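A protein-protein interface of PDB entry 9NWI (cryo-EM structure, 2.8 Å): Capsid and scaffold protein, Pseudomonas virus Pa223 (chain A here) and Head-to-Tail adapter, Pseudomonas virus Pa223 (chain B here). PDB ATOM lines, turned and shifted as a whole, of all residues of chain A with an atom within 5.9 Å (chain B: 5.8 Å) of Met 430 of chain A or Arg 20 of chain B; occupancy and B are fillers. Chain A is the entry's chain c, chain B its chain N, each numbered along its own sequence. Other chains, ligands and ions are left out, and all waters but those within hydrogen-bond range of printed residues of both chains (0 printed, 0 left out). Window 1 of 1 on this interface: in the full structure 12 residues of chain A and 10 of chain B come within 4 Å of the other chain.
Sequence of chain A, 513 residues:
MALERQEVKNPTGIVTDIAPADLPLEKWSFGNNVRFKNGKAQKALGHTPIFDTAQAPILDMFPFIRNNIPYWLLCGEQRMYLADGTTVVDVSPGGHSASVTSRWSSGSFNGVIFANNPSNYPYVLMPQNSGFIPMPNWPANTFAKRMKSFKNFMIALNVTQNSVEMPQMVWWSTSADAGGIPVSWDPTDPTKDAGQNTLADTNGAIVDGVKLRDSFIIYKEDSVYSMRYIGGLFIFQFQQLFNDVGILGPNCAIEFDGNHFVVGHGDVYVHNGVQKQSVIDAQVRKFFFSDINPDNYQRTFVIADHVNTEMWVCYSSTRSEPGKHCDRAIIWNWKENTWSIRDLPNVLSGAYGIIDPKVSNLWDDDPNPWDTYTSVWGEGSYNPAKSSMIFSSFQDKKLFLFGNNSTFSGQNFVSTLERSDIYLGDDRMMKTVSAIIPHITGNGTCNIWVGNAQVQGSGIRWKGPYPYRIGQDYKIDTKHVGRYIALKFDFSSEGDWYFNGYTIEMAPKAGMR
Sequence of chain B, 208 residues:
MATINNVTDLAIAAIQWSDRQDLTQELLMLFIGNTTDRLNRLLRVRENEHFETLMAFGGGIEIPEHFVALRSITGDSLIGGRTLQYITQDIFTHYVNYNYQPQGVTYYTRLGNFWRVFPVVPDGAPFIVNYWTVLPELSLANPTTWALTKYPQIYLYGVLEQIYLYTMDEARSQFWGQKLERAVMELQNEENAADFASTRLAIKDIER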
ATOM      1  N   ASP A 426      33.943 -20.550 -39.509  1.00  0.00           N
ATOM      2  CA  ASP A 426      33.107 -21.380 -38.645  1.00  0.00           C
ATOM      3  C   ASP A 426      31.704 -20.786 -38.645  1.00  0.00           C
ATOM      4  O   ASP A 426      31.459 -19.759 -38.005  1.00  0.00           O
ATOM      5  CB  ASP A 426      33.677 -21.457 -37.234  1.00  0.00           C
ATOM      6  CG  ASP A 426      32.715 -22.090 -36.254  1.00  0.00           C
ATOM      7  OD1 ASP A 426      32.705 -23.334 -36.149  1.00  0.00           O
ATOM      8  OD2 ASP A 426      31.964 -21.347 -35.591  1.00  0.00           O
ATOM      9  N   ARG A 428      28.828 -22.430 -37.698  1.00  0.00           N
ATOM     10  CA  ARG A 428      27.903 -23.157 -36.839  1.00  0.00           C
ATOM     11  C   ARG A 428      27.881 -22.618 -35.419  1.00  0.00           C
ATOM     12  O   ARG A 428      26.808 -22.282 -34.908  1.00  0.00           O
ATOM     13  CB  ARG A 428      28.253 -24.652 -36.823  1.00  0.00           C
ATOM     14  CG  ARG A 428      27.189 -25.516 -36.174  1.00  0.00           C
ATOM     15  CD  ARG A 428      25.823 -25.207 -36.756  1.00  0.00           C
ATOM     16  NE  ARG A 428      24.754 -25.353 -35.775  1.00  0.00           N
ATOM     17  CZ  ARG A 428      24.169 -26.501 -35.470  1.00  0.00           C
ATOM     18  NH1 ARG A 428      24.530 -27.634 -36.046  1.00  0.00           N
ATOM     19  NH2 ARG A 428      23.194 -26.511 -34.567  1.00  0.00           N
ATOM     20  N   MET A 429      29.034 -22.516 -34.770  1.00  0.00           N
ATOM     21  CA  MET A 429      29.089 -22.045 -33.398  1.00  0.00           C
ATOM     22  C   MET A 429      28.895 -20.535 -33.338  1.00  0.00           C
ATOM     23  O   MET A 429      28.942 -19.832 -34.349  1.00  0.00           O
ATOM     24  CB  MET A 429      30.418 -22.425 -32.748  1.00  0.00           C
ATOM     25  CG  MET A 429      30.877 -23.837 -33.051  1.00  0.00           C
ATOM     26  SD  MET A 429      30.057 -25.053 -32.008  1.00  0.00           S
ATOM     27  CE  MET A 429      30.794 -26.568 -32.608  1.00  0.00           C
ATOM     28  N   MET A 430      28.670 -20.038 -32.126  1.00  0.00           N
ATOM     29  CA  MET A 430      28.472 -18.618 -31.884  1.00  0.00           C
ATOM     30  C   MET A 430      29.732 -18.004 -31.295  1.00  0.00           C
ATOM     31  O   MET A 430      30.382 -18.601 -30.434  1.00  0.00           O
ATOM     32  CB  MET A 430      27.297 -18.384 -30.939  1.00  0.00           C
ATOM     33  CG  MET A 430      26.043 -19.134 -31.310  1.00  0.00           C
ATOM     34  SD  MET A 430      24.580 -18.160 -30.943  1.00  0.00           S
ATOM     35  CE  MET A 430      24.461 -17.184 -32.433  1.00  0.00           C
ATOM     36  N   LYS A 431      30.066 -16.808 -31.759  1.00  0.00           N
ATOM     37  CA  LYS A 431      31.231 -16.079 -31.288  1.00  0.00           C
ATOM     38  C   LYS A 431      30.833 -15.112 -30.180  1.00  0.00           C
ATOM     39  O   LYS A 431      29.654 -14.826 -29.968  1.00  0.00           O
ATOM     40  CB  LYS A 431      31.889 -15.327 -32.443  1.00  0.00           C
ATOM     41  CG  LYS A 431      32.570 -16.242 -33.442  1.00  0.00           C
ATOM     42  CD  LYS A 431      31.810 -16.289 -34.752  1.00  0.00           C
ATOM     43  CE  LYS A 431      32.087 -17.581 -35.497  1.00  0.00           C
ATOM     44  NZ  LYS A 431      30.845 -18.171 -36.058  1.00  0.00           N
ATOM     45  N   THR A 432      31.838 -14.610 -29.468  1.00  0.00           N
ATOM     46  CA  THR A 432      31.612 -13.760 -28.306  1.00  0.00           C
ATOM     47  C   THR A 432      31.990 -12.305 -28.522  1.00  0.00           C
ATOM     48  O   THR A 432      31.238 -11.420 -28.113  1.00  0.00           O
ATOM     49  CB  THR A 432      32.382 -14.300 -27.100  1.00  0.00           C
ATOM     50  OG1 THR A 432      32.289 -15.729 -27.079  1.00  0.00           O
ATOM     51  CG2 THR A 432      31.799 -13.747 -25.814  1.00  0.00           C
ATOM     52  N   ASN A 452      25.216  -8.424 -34.894  1.00  0.00           N
ATOM     53  CA  ASN A 452      25.277  -9.836 -35.229  1.00  0.00           C
ATOM     54  C   ASN A 452      24.041 -10.232 -36.019  1.00  0.00           C
ATOM     55  O   ASN A 452      22.982  -9.608 -35.921  1.00  0.00           O
ATOM     56  CB  ASN A 452      25.393 -10.714 -33.981  1.00  0.00           C
ATOM     57  CG  ASN A 452      24.048 -11.171 -33.466  1.00  0.00           C
ATOM     58  OD1 ASN A 452      23.566 -12.243 -33.824  1.00  0.00           O
ATOM     59  ND2 ASN A 452      23.427 -10.354 -32.629  1.00  0.00           N
ATOM     60  N   ALA A 453      24.199 -11.286 -36.808  1.00  0.00           N
ATOM     61  CA  ALA A 453      23.118 -11.880 -37.578  1.00  0.00           C
ATOM     62  C   ALA A 453      23.150 -13.389 -37.394  1.00  0.00           C
ATOM     63  O   ALA A 453      24.227 -13.989 -37.309  1.00  0.00           O
ATOM     64  CB  ALA A 453      23.227 -11.530 -39.062  1.00  0.00           C
ATOM     65  N   GLN A 454      21.967 -13.995 -37.333  1.00  0.00           N
ATOM     66  CA  GLN A 454      21.854 -15.433 -37.136  1.00  0.00           C
ATOM     67  C   GLN A 454      21.768 -16.210 -38.438  1.00  0.00           C
ATOM     68  O   GLN A 454      22.158 -17.381 -38.472  1.00  0.00           O
ATOM     69  CB  GLN A 454      20.624 -15.753 -36.285  1.00  0.00           C
ATOM     70  CG  GLN A 454      20.582 -15.009 -34.971  1.00  0.00           C
ATOM     71  CD  GLN A 454      21.562 -15.565 -33.967  1.00  0.00           C
ATOM     72  OE1 GLN A 454      21.498 -16.740 -33.608  1.00  0.00           O
ATOM     73  NE2 GLN A 454      22.480 -14.727 -33.510  1.00  0.00           N
ATOM     74  N   VAL A 481      27.233 -11.662 -28.376  1.00  0.00           N
ATOM     75  CA  VAL A 481      27.177 -13.044 -28.833  1.00  0.00           C
ATOM     76  C   VAL A 481      26.360 -13.109 -30.114  1.00  0.00           C
ATOM     77  O   VAL A 481      25.252 -12.568 -30.183  1.00  0.00           O
ATOM     78  CB  VAL A 481      26.576 -13.954 -27.752  1.00  0.00           C
ATOM     79  CG1 VAL A 481      26.727 -15.408 -28.148  1.00  0.00           C
ATOM     80  CG2 VAL A 481      27.241 -13.692 -26.418  1.00  0.00           C
ATOM     81  N   GLY A 482      26.904 -13.772 -31.129  1.00  0.00           N
ATOM     82  CA  GLY A 482      26.203 -13.908 -32.393  1.00  0.00           C
ATOM     83  C   GLY A 482      26.921 -14.885 -33.295  1.00  0.00           C
ATOM     84  O   GLY A 482      28.022 -15.352 -32.991  1.00  0.00           O
ATOM     85  N   ARG A 483      26.276 -15.189 -34.419  1.00  0.00           N
ATOM     86  CA  ARG A 483      26.831 -16.139 -35.373  1.00  0.00           C
ATOM     87  C   ARG A 483      27.652 -15.451 -36.458  1.00  0.00           C
ATOM     88  O   ARG A 483      28.767 -15.883 -36.761  1.00  0.00           O
ATOM     89  CB  ARG A 483      25.711 -16.968 -36.004  1.00  0.00           C
ATOM     90  CG  ARG A 483      26.193 -18.251 -36.652  1.00  0.00           C
ATOM     91  CD  ARG A 483      25.031 -19.112 -37.105  1.00  0.00           C
ATOM     92  NE  ARG A 483      24.717 -20.157 -36.140  1.00  0.00           N
ATOM     93  CZ  ARG A 483      23.493 -20.438 -35.716  1.00  0.00           C
ATOM     94  NH1 ARG A 483      22.440 -19.769 -36.152  1.00  0.00           N
ATOM     95  NH2 ARG A 483      23.322 -21.417 -34.833  1.00  0.00           N
ATOM     96  N   PRO A 508      36.114 -17.470 -25.655  1.00  0.00           N
ATOM     97  CA  PRO A 508      35.747 -18.788 -26.186  1.00  0.00           C
ATOM     98  C   PRO A 508      34.285 -18.838 -26.598  1.00  0.00           C
ATOM     99  O   PRO A 508      33.440 -18.117 -26.063  1.00  0.00           O
ATOM    100  CB  PRO A 508      36.033 -19.739 -25.016  1.00  0.00           C
ATOM    101  CG  PRO A 508      36.255 -18.860 -23.826  1.00  0.00           C
ATOM    102  CD  PRO A 508      36.817 -17.598 -24.369  1.00  0.00           C
ATOM    103  N   LYS A 509      34.000 -19.698 -27.574  1.00  0.00           N
ATOM    104  CA  LYS A 509      32.679 -19.765 -28.180  1.00  0.00           C
ATOM    105  C   LYS A 509      31.609 -20.066 -27.134  1.00  0.00           C
ATOM    106  O   LYS A 509      31.890 -20.527 -26.027  1.00  0.00           O
ATOM    107  CB  LYS A 509      32.653 -20.823 -29.279  1.00  0.00           C
ATOM    108  CG  LYS A 509      33.196 -20.335 -30.607  1.00  0.00           C
ATOM    109  CD  LYS A 509      33.779 -21.474 -31.419  1.00  0.00           C
ATOM    110  CE  LYS A 509      34.610 -20.949 -32.574  1.00  0.00           C
ATOM    111  NZ  LYS A 509      35.384 -19.744 -32.183  1.00  0.00           N
ATOM    112  N   ALA A 510      30.360 -19.807 -27.510  1.00  0.00           N
ATOM    113  CA  ALA A 510      29.224 -19.862 -26.599  1.00  0.00           C
ATOM    114  C   ALA A 510      28.166 -20.815 -27.124  1.00  0.00           C
ATOM    115  O   ALA A 510      26.973 -20.510 -27.159  1.00  0.00           O
ATOM    116  CB  ALA A 510      28.632 -18.475 -26.382  1.00  0.00           C
ATOM    117  N   GLY A 511      28.598 -21.995 -27.547  1.00  0.00           N
ATOM    118  CA  GLY A 511      27.692 -23.015 -28.032  1.00  0.00           C
ATOM    119  C   GLY A 511      27.344 -22.818 -29.492  1.00  0.00           C
ATOM    120  O   GLY A 511      27.714 -21.831 -30.136  1.00  0.00           O
ATOM    121  N   MET A 512      26.602 -23.788 -30.014  1.00  0.00           N
ATOM    122  CA  MET A 512      26.191 -23.777 -31.407  1.00  0.00           C
ATOM    123  C   MET A 512      24.724 -23.439 -31.615  1.00  0.00           C
ATOM    124  O   MET A 512      24.133 -23.888 -32.602  1.00  0.00           O
ATOM    125  CB  MET A 512      26.556 -25.114 -32.075  1.00  0.00           C
ATOM    126  CG  MET A 512      25.655 -26.320 -31.842  1.00  0.00           C
ATOM    127  SD  MET A 512      26.746 -27.756 -31.762  1.00  0.00           S
ATOM    128  CE  MET A 512      25.726 -28.981 -30.962  1.00  0.00           C
ATOM    129  N   ARG A 513      24.136 -22.626 -30.748  1.00  0.00           N
ATOM    130  CA  ARG A 513      22.785 -22.131 -30.958  1.00  0.00           C
ATOM    131  C   ARG A 513      22.582 -20.757 -30.329  1.00  0.00           C
ATOM    132  O   ARG A 513      23.055 -20.479 -29.228  1.00  0.00           O
ATOM    133  CB  ARG A 513      21.770 -23.116 -30.397  1.00  0.00           C
ATOM    134  CG  ARG A 513      20.356 -22.608 -30.441  1.00  0.00           C
ATOM    135  CD  ARG A 513      19.394 -23.756 -30.440  1.00  0.00           C
ATOM    136  NE  ARG A 513      19.086 -24.185 -29.081  1.00  0.00           N
ATOM    137  CZ  ARG A 513      17.919 -23.995 -28.487  1.00  0.00           C
ATOM    138  NH1 ARG A 513      16.925 -23.375 -29.101  1.00  0.00           N
ATOM    139  NH2 ARG A 513      17.740 -24.445 -27.251  1.00  0.00           N
ATOM    140  OXT ARG A 513      21.932 -19.889 -30.911  1.00  0.00           O
ATOM    141  N   ALA B  14      19.319 -11.781 -16.080  1.00  0.00           N
ATOM    142  CA  ALA B  14      19.723 -12.975 -16.814  1.00  0.00           C
ATOM    143  C   ALA B  14      19.966 -12.659 -18.282  1.00  0.00           C
ATOM    144  O   ALA B  14      20.959 -13.112 -18.868  1.00  0.00           O
ATOM    145  CB  ALA B  14      18.664 -14.064 -16.668  1.00  0.00           C
ATOM    146  N   ILE B  15      19.077 -11.873 -18.890  1.00  0.00           N
ATOM    147  CA  ILE B  15      19.263 -11.487 -20.286  1.00  0.00           C
ATOM    148  C   ILE B  15      20.542 -10.680 -20.447  1.00  0.00           C
ATOM    149  O   ILE B  15      21.316 -10.895 -21.386  1.00  0.00           O
ATOM    150  CB  ILE B  15      18.036 -10.711 -20.794  1.00  0.00           C
ATOM    151  CG1 ILE B  15      16.802 -11.614 -20.807  1.00  0.00           C
ATOM    152  CG2 ILE B  15      18.303 -10.130 -22.169  1.00  0.00           C
ATOM    153  CD1 ILE B  15      16.649 -12.424 -22.066  1.00  0.00           C
ATOM    154  N   SER B  18      23.668 -13.070 -19.992  1.00  0.00           N
ATOM    155  CA  SER B  18      23.839 -14.050 -21.057  1.00  0.00           C
ATOM    156  C   SER B  18      23.888 -13.425 -22.442  1.00  0.00           C
ATOM    157  O   SER B  18      24.335 -14.086 -23.384  1.00  0.00           O
ATOM    158  CB  SER B  18      22.710 -15.078 -21.010  1.00  0.00           C
ATOM    159  OG  SER B  18      21.572 -14.600 -21.700  1.00  0.00           O
ATOM    160  N   ASP B  19      23.429 -12.182 -22.590  1.00  0.00           N
ATOM    161  CA  ASP B  19      23.365 -11.428 -23.839  1.00  0.00           C
ATOM    162  C   ASP B  19      22.375 -12.015 -24.840  1.00  0.00           C
ATOM    163  O   ASP B  19      22.221 -11.459 -25.930  1.00  0.00           O
ATOM    164  CB  ASP B  19      24.738 -11.297 -24.517  1.00  0.00           C
ATOM    165  CG  ASP B  19      24.779 -10.178 -25.537  1.00  0.00           C
ATOM    166  OD1 ASP B  19      24.416  -9.038 -25.184  1.00  0.00           O
ATOM    167  OD2 ASP B  19      25.167 -10.441 -26.694  1.00  0.00           O
ATOM    168  N   ARG B  20      21.689 -13.104 -24.508  1.00  0.00           N
ATOM    169  CA  ARG B  20      20.743 -13.726 -25.431  1.00  0.00           C
ATOM    170  C   ARG B  20      19.427 -12.964 -25.364  1.00  0.00           C
ATOM    171  O   ARG B  20      18.546 -13.269 -24.562  1.00  0.00           O
ATOM    172  CB  ARG B  20      20.554 -15.198 -25.094  1.00  0.00           C
ATOM    173  CG  ARG B  20      21.842 -15.924 -24.776  1.00  0.00           C
ATOM    174  CD  ARG B  20      22.643 -16.184 -26.034  1.00  0.00           C
ATOM    175  NE  ARG B  20      21.777 -16.419 -27.182  1.00  0.00           N
ATOM    176  CZ  ARG B  20      21.973 -17.371 -28.083  1.00  0.00           C
ATOM    177  NH1 ARG B  20      23.001 -18.198 -28.000  1.00  0.00           N
ATOM    178  NH2 ARG B  20      21.115 -17.496 -29.090  1.00  0.00           N
ATOM    179  N   GLN B  21      19.290 -11.959 -26.225  1.00  0.00           N
ATOM    180  CA  GLN B  21      18.071 -11.162 -26.271  1.00  0.00           C
ATOM    181  C   GLN B  21      16.938 -11.851 -27.016  1.00  0.00           C
ATOM    182  O   GLN B  21      15.815 -11.337 -27.010  1.00  0.00           O
ATOM    183  CB  GLN B  21      18.354  -9.807 -26.919  1.00  0.00           C
ATOM    184  CG  GLN B  21      19.597  -9.125 -26.393  1.00  0.00           C
ATOM    185  CD  GLN B  21      19.384  -7.650 -26.139  1.00  0.00           C
ATOM    186  OE1 GLN B  21      18.295  -7.122 -26.355  1.00  0.00           O
ATOM    187  NE2 GLN B  21      20.427  -6.973 -25.676  1.00  0.00           N
ATOM    188  N   ASP B  22      17.199 -12.990 -27.652  1.00  0.00           N
ATOM    189  CA  ASP B  22      16.172 -13.698 -28.401  1.00  0.00           C
ATOM    190  C   ASP B  22      15.286 -14.570 -27.523  1.00  0.00           C
ATOM    191  O   ASP B  22      14.294 -15.111 -28.021  1.00  0.00           O
ATOM    192  CB  ASP B  22      16.821 -14.563 -29.481  1.00  0.00           C
ATOM    193  CG  ASP B  22      18.093 -15.227 -29.001  1.00  0.00           C
ATOM    194  OD1 ASP B  22      18.936 -14.527 -28.401  1.00  0.00           O
ATOM    195  OD2 ASP B  22      18.251 -16.445 -29.218  1.00  0.00           O
ATOM    196  N   LEU B  23      15.613 -14.723 -26.244  1.00  0.00           N
ATOM    197  CA  LEU B  23      14.821 -15.574 -25.369  1.00  0.00           C
ATOM    198  C   LEU B  23      13.504 -14.894 -25.017  1.00  0.00           C
ATOM    199  O   LEU B  23      13.480 -13.722 -24.632  1.00  0.00           O
ATOM    200  CB  LEU B  23      15.603 -15.901 -24.100  1.00  0.00           C
ATOM    201  CG  LEU B  23      16.974 -16.537 -24.320  1.00  0.00           C
ATOM    202  CD1 LEU B  23      17.742 -16.614 -23.016  1.00  0.00           C
ATOM    203  CD2 LEU B  23      16.824 -17.913 -24.937  1.00  0.00           C
ATOM    204  N   ILE B 163      19.997 -21.573 -19.107  1.00  0.00           N
ATOM    205  CA  ILE B 163      20.155 -20.913 -20.400  1.00  0.00           C
ATOM    206  C   ILE B 163      21.252 -21.589 -21.207  1.00  0.00           C
ATOM    207  O   ILE B 163      21.085 -21.881 -22.396  1.00  0.00           O
ATOM    208  CB  ILE B 163      20.445 -19.415 -20.204  1.00  0.00           C
ATOM    209  CG1 ILE B 163      19.161 -18.661 -19.870  1.00  0.00           C
ATOM    210  CG2 ILE B 163      21.090 -18.830 -21.443  1.00  0.00           C
ATOM    211  CD1 ILE B 163      19.388 -17.215 -19.513  1.00  0.00           C
ATOM    212  N   THR B 167      21.084 -23.435 -24.957  1.00  0.00           N
ATOM    213  CA  THR B 167      21.862 -23.097 -26.140  1.00  0.00           C
ATOM    214  C   THR B 167      22.877 -24.173 -26.499  1.00  0.00           C
ATOM    215  O   THR B 167      23.693 -23.965 -27.401  1.00  0.00           O
ATOM    216  CB  THR B 167      22.571 -21.758 -25.950  1.00  0.00           C
ATOM    217  OG1 THR B 167      23.646 -21.913 -25.018  1.00  0.00           O
ATOM    218  CG2 THR B 167      21.603 -20.716 -25.428  1.00  0.00           C
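Thr 167 of chain B touches Met 512 of chain A.
Arg 513 of chain A touches Thr 167 of chain B (O to CB, 3.6 Å).
N of Val 481 of chain A sits at hydrogen-bond distance from OD2 of Asp 19 of chain B (2.9 Å).
NH1 of Arg 20 of chain B lies within hydrogen-bond range of SD of Met 430 of chain A, 3.3 Å away.
The guanidinium group (NH1) of Arg 20 of chain B is in salt-bridge range of the chain-end carboxylate (O) of Arg 513 of chain A.
N of Arg 20 of chain B lies close to OG of Ser 18 of chain B.
The guanidinium group (NH2) of Arg 20 of chain B lies within salt-bridge range of the side-chain carboxylate (OD2) of Asp 22 of chain B, at 3.1 Å.
NH2 of Arg 428 of chain A sits at hydrogen-bond distance from O of Met 512 of chain A (3.4 Å).
The backbone carbonyl oxygen (O) of Met 430 of chain A is in hydrogen-bond range of the backbone NH (N) of Ala 510 of chain A.
O of Gly 511 of chain A is in hydrogen-bond range of N of Met 430 of chain A (2.8 Å).
O of Met 512 of chain A lies within hydrogen-bond range of NH2 of Arg 483 of chain A (3.4 Å).
Of the 10 printed residues of chain B, 3 touch a printed residue of chain A.
Along chain B the printed residues that touch a printed residue of chain A span positions 19 to 167.
Of the 18 printed residues of chain A, 4 touch a printed residue of chain B.
Printed residues of chain A that touch a printed residue of chain B: Met 430, Val 481, Met 512 and Arg 513.
Hydrophobic or aromatic side chains of chain A within 4 Å of the printed part of chain B: Met 430 and Val 481.
Among the printed residues, 5 pairs touch across the chains.
Among the printed residues, no Asp or Glu carboxylate lies within 4 Å of a Lys or Arg side-chain nitrogen of the other chain.
Of chain B, only Arg 20 (3.3 Å) comes within 4 Å of Met 430 of chain A.
Arg 20 of chain B touches just these residues of chain A: Met 430 (3.3 Å) and Arg 513 (2.6 Å).
Of the printed residues of chain B, Met 512 of chain A touches Thr 167 (3.9 Å).
Of the printed residues of chain B, Arg 513 of chain A touches Arg 20 (2.6 Å) and Thr 167 (3.6 Å).
Of the printed residues of chain A, Thr 167 of chain B touches Met 512 and Arg 513.
Printed residues of chain A within 4 Å of Asp 19 of chain B: Val 481 (2.9 Å).
Printed residues of chain B within 4 Å of Val 481 of chain A: Asp 19.
Asp 426 of chain A touches none of the printed residues of chain B.
The nearest printed residue of chain B that does not touch Met 430 of chain A is Thr 167 of chain B (6.5 Å).
The nearest residue of chain A that does not touch Arg 20 of chain B is Gln 454 of chain A (4.6 Å).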
